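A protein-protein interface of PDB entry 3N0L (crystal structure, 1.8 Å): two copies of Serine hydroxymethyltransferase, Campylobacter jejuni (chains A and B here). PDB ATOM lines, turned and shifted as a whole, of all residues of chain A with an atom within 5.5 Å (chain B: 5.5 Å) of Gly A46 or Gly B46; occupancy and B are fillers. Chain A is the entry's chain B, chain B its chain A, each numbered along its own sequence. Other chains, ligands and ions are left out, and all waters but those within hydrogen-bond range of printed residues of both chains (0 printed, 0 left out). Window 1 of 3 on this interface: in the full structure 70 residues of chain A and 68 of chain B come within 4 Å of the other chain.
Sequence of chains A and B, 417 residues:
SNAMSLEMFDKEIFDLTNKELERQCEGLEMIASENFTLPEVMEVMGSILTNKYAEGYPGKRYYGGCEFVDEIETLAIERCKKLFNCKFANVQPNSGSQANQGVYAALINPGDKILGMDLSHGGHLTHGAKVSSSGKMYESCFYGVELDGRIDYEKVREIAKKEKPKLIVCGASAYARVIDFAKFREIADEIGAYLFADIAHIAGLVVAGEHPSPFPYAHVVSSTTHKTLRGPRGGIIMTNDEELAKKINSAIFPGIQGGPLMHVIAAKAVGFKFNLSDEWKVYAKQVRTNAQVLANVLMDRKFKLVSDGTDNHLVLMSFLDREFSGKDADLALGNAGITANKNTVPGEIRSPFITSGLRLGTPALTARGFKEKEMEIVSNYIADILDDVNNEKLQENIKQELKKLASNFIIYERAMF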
ATOM      1  N   MET A  42       0.327 -21.861 -28.663  1.00  0.00           N
ATOM      2  CA  MET A  42       1.037 -23.080 -28.320  1.00  0.00           C
ATOM      3  C   MET A  42       1.576 -23.041 -26.901  1.00  0.00           C
ATOM      4  O   MET A  42       1.617 -24.071 -26.215  1.00  0.00           O
ATOM      5  CB  MET A  42       2.148 -23.348 -29.325  1.00  0.00           C
ATOM      6  CG  MET A  42       1.582 -23.905 -30.589  1.00  0.00           C
ATOM      7  SD  MET A  42       2.929 -24.146 -31.916  1.00  0.00           S
ATOM      8  CE  MET A  42       3.356 -22.297 -32.312  1.00  0.00           C
ATOM      9  N   GLU A  43       1.962 -21.858 -26.444  1.00  0.00           N
ATOM     10  CA  GLU A  43       2.520 -21.770 -25.108  1.00  0.00           C
ATOM     11  C   GLU A  43       1.498 -22.236 -24.095  1.00  0.00           C
ATOM     12  O   GLU A  43       1.816 -23.001 -23.193  1.00  0.00           O
ATOM     13  CB  GLU A  43       3.002 -20.357 -24.795  1.00  0.00           C
ATOM     14  CG  GLU A  43       4.215 -19.960 -25.600  1.00  0.00           C
ATOM     15  CD  GLU A  43       4.753 -18.605 -25.202  1.00  0.00           C
ATOM     16  OE1 GLU A  43       4.109 -17.931 -24.363  1.00  0.00           O
ATOM     17  OE2 GLU A  43       5.821 -18.218 -25.728  1.00  0.00           O
ATOM     18  N   VAL A  44       0.247 -21.825 -24.252  1.00  0.00           N
ATOM     19  CA  VAL A  44      -0.714 -22.197 -23.225  1.00  0.00           C
ATOM     20  C   VAL A  44      -1.175 -23.634 -23.374  1.00  0.00           C
ATOM     21  O   VAL A  44      -1.742 -24.193 -22.451  1.00  0.00           O
ATOM     22  CB  VAL A  44      -1.923 -21.237 -23.139  1.00  0.00           C
ATOM     23  CG1 VAL A  44      -2.895 -21.510 -24.261  1.00  0.00           C
ATOM     24  CG2 VAL A  44      -2.605 -21.387 -21.771  1.00  0.00           C
ATOM     25  N   MET A  45      -0.928 -24.240 -24.533  1.00  0.00           N
ATOM     26  CA  MET A  45      -1.335 -25.629 -24.718  1.00  0.00           C
ATOM     27  C   MET A  45      -0.459 -26.585 -23.954  1.00  0.00           C
ATOM     28  O   MET A  45      -0.916 -27.658 -23.562  1.00  0.00           O
ATOM     29  CB  MET A  45      -1.296 -26.012 -26.185  1.00  0.00           C
ATOM     30  CG  MET A  45      -1.943 -24.982 -27.058  1.00  0.00           C
ATOM     31  SD  MET A  45      -2.071 -25.696 -28.829  1.00  0.00           S
ATOM     32  CE  MET A  45      -3.203 -27.188 -28.321  1.00  0.00           C
ATOM     33  N   GLY A  46       0.804 -26.222 -23.764  1.00  0.00           N
ATOM     34  CA  GLY A  46       1.710 -27.084 -23.023  1.00  0.00           C
ATOM     35  C   GLY A  46       1.703 -26.739 -21.548  1.00  0.00           C
ATOM     36  O   GLY A  46       2.757 -26.521 -20.951  1.00  0.00           O
ATOM     37  N   SER A  47       0.514 -26.705 -20.951  1.00  0.00           N
ATOM     38  CA  SER A  47       0.376 -26.171 -19.599  1.00  0.00           C
ATOM     39  C   SER A  47      -0.250 -27.150 -18.632  1.00  0.00           C
ATOM     40  O   SER A  47      -0.793 -28.187 -19.026  1.00  0.00           O
ATOM     41  CB  SER A  47      -0.473 -24.884 -19.608  1.00  0.00           C
ATOM     42  OG  SER A  47      -1.835 -25.197 -19.855  1.00  0.00           O
ATOM     43  N   ILE A  48      -0.194 -26.802 -17.351  1.00  0.00           N
ATOM     44  CA  ILE A  48      -0.842 -27.621 -16.329  1.00  0.00           C
ATOM     45  C   ILE A  48      -2.381 -27.643 -16.403  1.00  0.00           C
ATOM     46  O   ILE A  48      -3.029 -28.325 -15.606  1.00  0.00           O
ATOM     47  CB  ILE A  48      -0.343 -27.246 -14.922  1.00  0.00           C
ATOM     48  CG1 ILE A  48      -0.502 -25.738 -14.665  1.00  0.00           C
ATOM     49  CG2 ILE A  48       1.126 -27.599 -14.793  1.00  0.00           C
ATOM     50  CD1 ILE A  48      -1.931 -25.272 -14.503  1.00  0.00           C
ATOM     51  N   HIS A 263      -6.658 -27.148 -21.613  1.00  0.00           N
ATOM     52  CA  HIS A 263      -5.496 -26.463 -22.174  1.00  0.00           C
ATOM     53  C   HIS A 263      -5.833 -26.010 -23.598  1.00  0.00           C
ATOM     54  O   HIS A 263      -5.376 -24.953 -24.056  1.00  0.00           O
ATOM     55  CB  HIS A 263      -4.235 -27.339 -22.139  1.00  0.00           C
ATOM     56  CG  HIS A 263      -4.303 -28.538 -23.036  1.00  0.00           C
ATOM     57  ND1 HIS A 263      -5.037 -29.659 -22.726  1.00  0.00           N
ATOM     58  CD2 HIS A 263      -3.732 -28.788 -24.239  1.00  0.00           C
ATOM     59  CE1 HIS A 263      -4.916 -30.553 -23.691  1.00  0.00           C
ATOM     60  NE2 HIS A 263      -4.133 -30.045 -24.625  1.00  0.00           N
ATOM     61  N   ALA A 415      10.635 -25.367 -32.052  1.00  0.00           N
ATOM     62  CA  ALA A 415       9.559 -26.304 -32.361  1.00  0.00           C
ATOM     63  C   ALA A 415       8.550 -26.387 -31.222  1.00  0.00           C
ATOM     64  O   ALA A 415       7.382 -26.715 -31.429  1.00  0.00           O
ATOM     65  CB  ALA A 415      10.133 -27.695 -32.654  1.00  0.00           C
ATOM     66  N   MET A 416       9.020 -26.105 -30.014  1.00  0.00           N
ATOM     67  CA  MET A 416       8.170 -26.226 -28.838  1.00  0.00           C
ATOM     68  C   MET A 416       8.138 -24.945 -28.030  1.00  0.00           C
ATOM     69  O   MET A 416       9.164 -24.305 -27.809  1.00  0.00           O
ATOM     70  CB  MET A 416       8.641 -27.380 -27.974  1.00  0.00           C
ATOM     71  CG  MET A 416       8.327 -28.707 -28.603  1.00  0.00           C
ATOM     72  SD  MET A 416       9.557 -30.052 -28.007  1.00  0.00           S
ATOM     73  CE  MET A 416      11.062 -29.646 -29.188  1.00  0.00           C
ATOM     74  N   PHE A 417       6.943 -24.598 -27.573  1.00  0.00           N
ATOM     75  CA  PHE A 417       6.709 -23.317 -26.937  1.00  0.00           C
ATOM     76  C   PHE A 417       6.206 -23.485 -25.508  1.00  0.00           C
ATOM     77  O   PHE A 417       6.322 -22.569 -24.696  1.00  0.00           O
ATOM     78  CB  PHE A 417       5.726 -22.504 -27.780  1.00  0.00           C
ATOM     79  CG  PHE A 417       6.301 -22.057 -29.100  1.00  0.00           C
ATOM     80  CD1 PHE A 417       6.978 -20.855 -29.205  1.00  0.00           C
ATOM     81  CD2 PHE A 417       6.204 -22.864 -30.223  1.00  0.00           C
ATOM     82  CE1 PHE A 417       7.531 -20.449 -30.408  1.00  0.00           C
ATOM     83  CE2 PHE A 417       6.751 -22.457 -31.439  1.00  0.00           C
ATOM     84  CZ  PHE A 417       7.413 -21.248 -31.526  1.00  0.00           C
ATOM     85  OXT PHE A 417       5.692 -24.539 -25.128  1.00  0.00           O
ATOM     86  N   MET B  42       3.986 -32.353 -21.382  1.00  0.00           N
ATOM     87  CA  MET B  42       3.487 -31.024 -21.689  1.00  0.00           C
ATOM     88  C   MET B  42       4.376 -30.265 -22.672  1.00  0.00           C
ATOM     89  O   MET B  42       3.873 -29.522 -23.506  1.00  0.00           O
ATOM     90  CB  MET B  42       3.255 -30.237 -20.410  1.00  0.00           C
ATOM     91  CG  MET B  42       2.022 -30.748 -19.691  1.00  0.00           C
ATOM     92  SD  MET B  42       1.823 -29.830 -18.002  1.00  0.00           S
ATOM     93  CE  MET B  42       3.290 -30.673 -17.037  1.00  0.00           C
ATOM     94  N   GLU B  43       5.687 -30.460 -22.589  1.00  0.00           N
ATOM     95  CA  GLU B  43       6.589 -29.758 -23.500  1.00  0.00           C
ATOM     96  C   GLU B  43       6.210 -30.024 -24.957  1.00  0.00           C
ATOM     97  O   GLU B  43       6.091 -29.092 -25.773  1.00  0.00           O
ATOM     98  CB  GLU B  43       8.049 -30.145 -23.241  1.00  0.00           C
ATOM     99  CG  GLU B  43       8.617 -29.597 -21.934  1.00  0.00           C
ATOM    100  CD  GLU B  43      10.040 -30.065 -21.663  1.00  0.00           C
ATOM    101  OE1 GLU B  43      10.774 -30.325 -22.635  1.00  0.00           O
ATOM    102  OE2 GLU B  43      10.418 -30.182 -20.478  1.00  0.00           O
ATOM    103  N   VAL B  44       5.983 -31.288 -25.294  1.00  0.00           N
ATOM    104  CA  VAL B  44       5.736 -31.612 -26.693  1.00  0.00           C
ATOM    105  C   VAL B  44       4.303 -31.256 -27.119  1.00  0.00           C
ATOM    106  O   VAL B  44       3.996 -31.179 -28.299  1.00  0.00           O
ATOM    107  CB  VAL B  44       6.095 -33.090 -27.019  1.00  0.00           C
ATOM    108  CG1 VAL B  44       4.972 -34.020 -26.580  1.00  0.00           C
ATOM    109  CG2 VAL B  44       6.398 -33.245 -28.518  1.00  0.00           C
ATOM    110  N   MET B  45       3.423 -31.028 -26.153  1.00  0.00           N
ATOM    111  CA  MET B  45       2.044 -30.659 -26.459  1.00  0.00           C
ATOM    112  C   MET B  45       1.950 -29.254 -27.019  1.00  0.00           C
ATOM    113  O   MET B  45       1.091 -28.967 -27.851  1.00  0.00           O
ATOM    114  CB  MET B  45       1.179 -30.766 -25.212  1.00  0.00           C
ATOM    115  CG  MET B  45       1.169 -32.161 -24.643  1.00  0.00           C
ATOM    116  SD  MET B  45       0.112 -32.242 -23.039  1.00  0.00           S
ATOM    117  CE  MET B  45      -1.641 -31.931 -23.832  1.00  0.00           C
ATOM    118  N   GLY B  46       2.834 -28.381 -26.557  1.00  0.00           N
ATOM    119  CA  GLY B  46       2.845 -27.010 -27.018  1.00  0.00           C
ATOM    120  C   GLY B  46       3.787 -26.832 -28.189  1.00  0.00           C
ATOM    121  O   GLY B  46       4.657 -25.972 -28.163  1.00  0.00           O
ATOM    122  N   SER B  47       3.594 -27.634 -29.230  1.00  0.00           N
ATOM    123  CA  SER B  47       4.547 -27.687 -30.329  1.00  0.00           C
ATOM    124  C   SER B  47       3.884 -27.472 -31.678  1.00  0.00           C
ATOM    125  O   SER B  47       2.649 -27.500 -31.799  1.00  0.00           O
ATOM    126  CB  SER B  47       5.277 -29.030 -30.334  1.00  0.00           C
ATOM    127  OG  SER B  47       4.404 -30.046 -30.799  1.00  0.00           O
ATOM    128  N   ILE B  48       4.725 -27.293 -32.695  1.00  0.00           N
ATOM    129  CA  ILE B  48       4.272 -27.080 -34.063  1.00  0.00           C
ATOM    130  C   ILE B  48       3.592 -28.293 -34.709  1.00  0.00           C
ATOM    131  O   ILE B  48       3.124 -28.211 -35.853  1.00  0.00           O
ATOM    132  CB  ILE B  48       5.421 -26.527 -34.958  1.00  0.00           C
ATOM    133  CG1 ILE B  48       6.680 -27.408 -34.868  1.00  0.00           C
ATOM    134  CG2 ILE B  48       5.784 -25.119 -34.499  1.00  0.00           C
ATOM    135  CD1 ILE B  48       6.541 -28.815 -35.445  1.00  0.00           C
ATOM    136  N   HIS B 263      -0.028 -33.268 -31.969  1.00  0.00           N
ATOM    137  CA  HIS B 263       0.733 -32.841 -30.797  1.00  0.00           C
ATOM    138  C   HIS B 263       0.376 -33.707 -29.587  1.00  0.00           C
ATOM    139  O   HIS B 263       1.231 -34.023 -28.746  1.00  0.00           O
ATOM    140  CB  HIS B 263       0.548 -31.332 -30.535  1.00  0.00           C
ATOM    141  CG  HIS B 263      -0.797 -30.954 -29.986  1.00  0.00           C
ATOM    142  ND1 HIS B 263      -1.904 -30.776 -30.782  1.00  0.00           N
ATOM    143  CD2 HIS B 263      -1.198 -30.673 -28.723  1.00  0.00           C
ATOM    144  CE1 HIS B 263      -2.932 -30.412 -30.037  1.00  0.00           C
ATOM    145  NE2 HIS B 263      -2.534 -30.356 -28.780  1.00  0.00           N
ATOM    146  N   ALA B 415       3.975 -23.084 -14.731  1.00  0.00           N
ATOM    147  CA  ALA B 415       2.666 -23.506 -15.229  1.00  0.00           C
ATOM    148  C   ALA B 415       2.712 -23.973 -16.674  1.00  0.00           C
ATOM    149  O   ALA B 415       1.900 -24.808 -17.087  1.00  0.00           O
ATOM    150  CB  ALA B 415       1.654 -22.368 -15.094  1.00  0.00           C
ATOM    151  N   MET B 416       3.650 -23.425 -17.440  1.00  0.00           N
ATOM    152  CA  MET B 416       3.742 -23.735 -18.865  1.00  0.00           C
ATOM    153  C   MET B 416       5.109 -24.249 -19.288  1.00  0.00           C
ATOM    154  O   MET B 416       6.145 -23.689 -18.917  1.00  0.00           O
ATOM    155  CB  MET B 416       3.350 -22.521 -19.685  1.00  0.00           C
ATOM    156  CG  MET B 416       1.893 -22.206 -19.512  1.00  0.00           C
ATOM    157  SD  MET B 416       1.492 -20.430 -20.088  1.00  0.00           S
ATOM    158  CE  MET B 416       1.416 -19.535 -18.358  1.00  0.00           C
ATOM    159  N   PHE B 417       5.087 -25.329 -20.061  1.00  0.00           N
ATOM    160  CA  PHE B 417       6.294 -26.051 -20.444  1.00  0.00           C
ATOM    161  C   PHE B 417       6.536 -26.006 -21.951  1.00  0.00           C
ATOM    162  O   PHE B 417       7.671 -26.172 -22.397  1.00  0.00           O
ATOM    163  CB  PHE B 417       6.203 -27.497 -19.952  1.00  0.00           C
ATOM    164  CG  PHE B 417       6.194 -27.608 -18.461  1.00  0.00           C
ATOM    165  CD1 PHE B 417       7.381 -27.742 -17.760  1.00  0.00           C
ATOM    166  CD2 PHE B 417       5.000 -27.526 -17.753  1.00  0.00           C
ATOM    167  CE1 PHE B 417       7.380 -27.825 -16.379  1.00  0.00           C
ATOM    168  CE2 PHE B 417       4.995 -27.605 -16.371  1.00  0.00           C
ATOM    169  CZ  PHE B 417       6.185 -27.757 -15.685  1.00  0.00           C
ATOM    170  OXT PHE B 417       5.619 -25.788 -22.747  1.00  0.00           O
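The side-chain sulfur (SD) of Met B42 lies within hydrogen-bond range of the backbone NH (N) of Ile A48, at 3.7 Å. The backbone carbonyl oxygen of Gly B46 is in hydrogen-bond range of the backbone NH of Phe A417 (2.7 Å). The backbone NH (N) of Ile B48 sits at hydrogen-bond distance from the side-chain sulfur (SD) of Met A42 (3.7 Å). N of Ile B48 is in hydrogen-bond range of O of Ala A415, 3.0 Å away. The backbone carbonyl oxygen of Ala B415 is in hydrogen-bond range of the backbone NH of Ile A48 (2.9 Å). The backbone carbonyl oxygen (O) of Gly A46 is in hydrogen-bond range of the backbone NH (N) of Phe B417 (2.8 Å). The chain-end carboxylate (OXT) of Phe A417 sits close to the chain-end carboxylate (OXT) of Phe B417 (2.7 Å). SD of Met A42 sits close to O of Ser B47 (3.4 Å). SD of Met B42 sits close to O of Ser A47, 3.3 Å away.
The backbone carbonyl oxygen (O) of Val B44 sits at hydrogen-bond distance from the side-chain hydroxyl (OG) of Ser B47, at 2.8 Å. O of Val A44 is in hydrogen-bond range of OG of Ser A47 (2.8 Å).
O of Met A42 touches CA of Gly B46, 3.3 Å away. Met A45 touches His B263. Met B42 touches Gly A46 (O to CA, 3.3 Å). N of Gly A46 touches CA of Gly B46 (3.9 Å). Met B416 touches Gly A46. CE of Met B45 touches NE2 of His A263, at 3.2 Å. Ala A415 touches Ser B47 (O to CA, 3.2 Å). CG of Met A416 touches O of Glu B43 (3.6 Å). O of Gly B46 touches CA of Met A416 (3.6 Å). CB of Ser B47 touches CG of Met A416 (3.5 Å).
Gly A46 touches just these residues of chain B: Met B42, Gly B46, Met B416 and Phe B417. Of the printed residues of chain A, Glu B43 touches Met A416. Printed residues of chain B within 4 Å of Met A42: Gly B46 (3.3 Å), Ser B47 (3.4 Å) and Ile B48 (3.7 Å). Of the printed residues of chain B, Phe A417 touches Gly B46 (2.7 Å) and Phe B417 (2.7 Å). Val A44 touches none of the printed residues of chain B. The nearest printed residue of chain A that does not touch Met B416 is Val A44 (4.2 Å).
Hydrophobic or aromatic side chains of chain B within 4 Å of the printed part of chain A: Met B42, Met B45, Ile B48, His B263, Met B416 and Phe B417. Among the printed residues, no Asp or Glu carboxylate lies within 4 Å of a Lys or Arg side-chain nitrogen of the other chain.
Met A42 touches Ser B47, and with the chains exchanged Ser A47 touches Met B42. Met A42 touches Ile B48, and with the chains exchanged Ile A48 touches Met B42. Met A45 touches His B263, and with the chains exchanged His A263 touches Met B45. Gly A46 touches Phe B417, and with the chains exchanged Phe A417 touches Gly B46. Of the 22 pairs that touch across the chains among the printed residues, 22 have their exchanged pair printed and touching as well.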
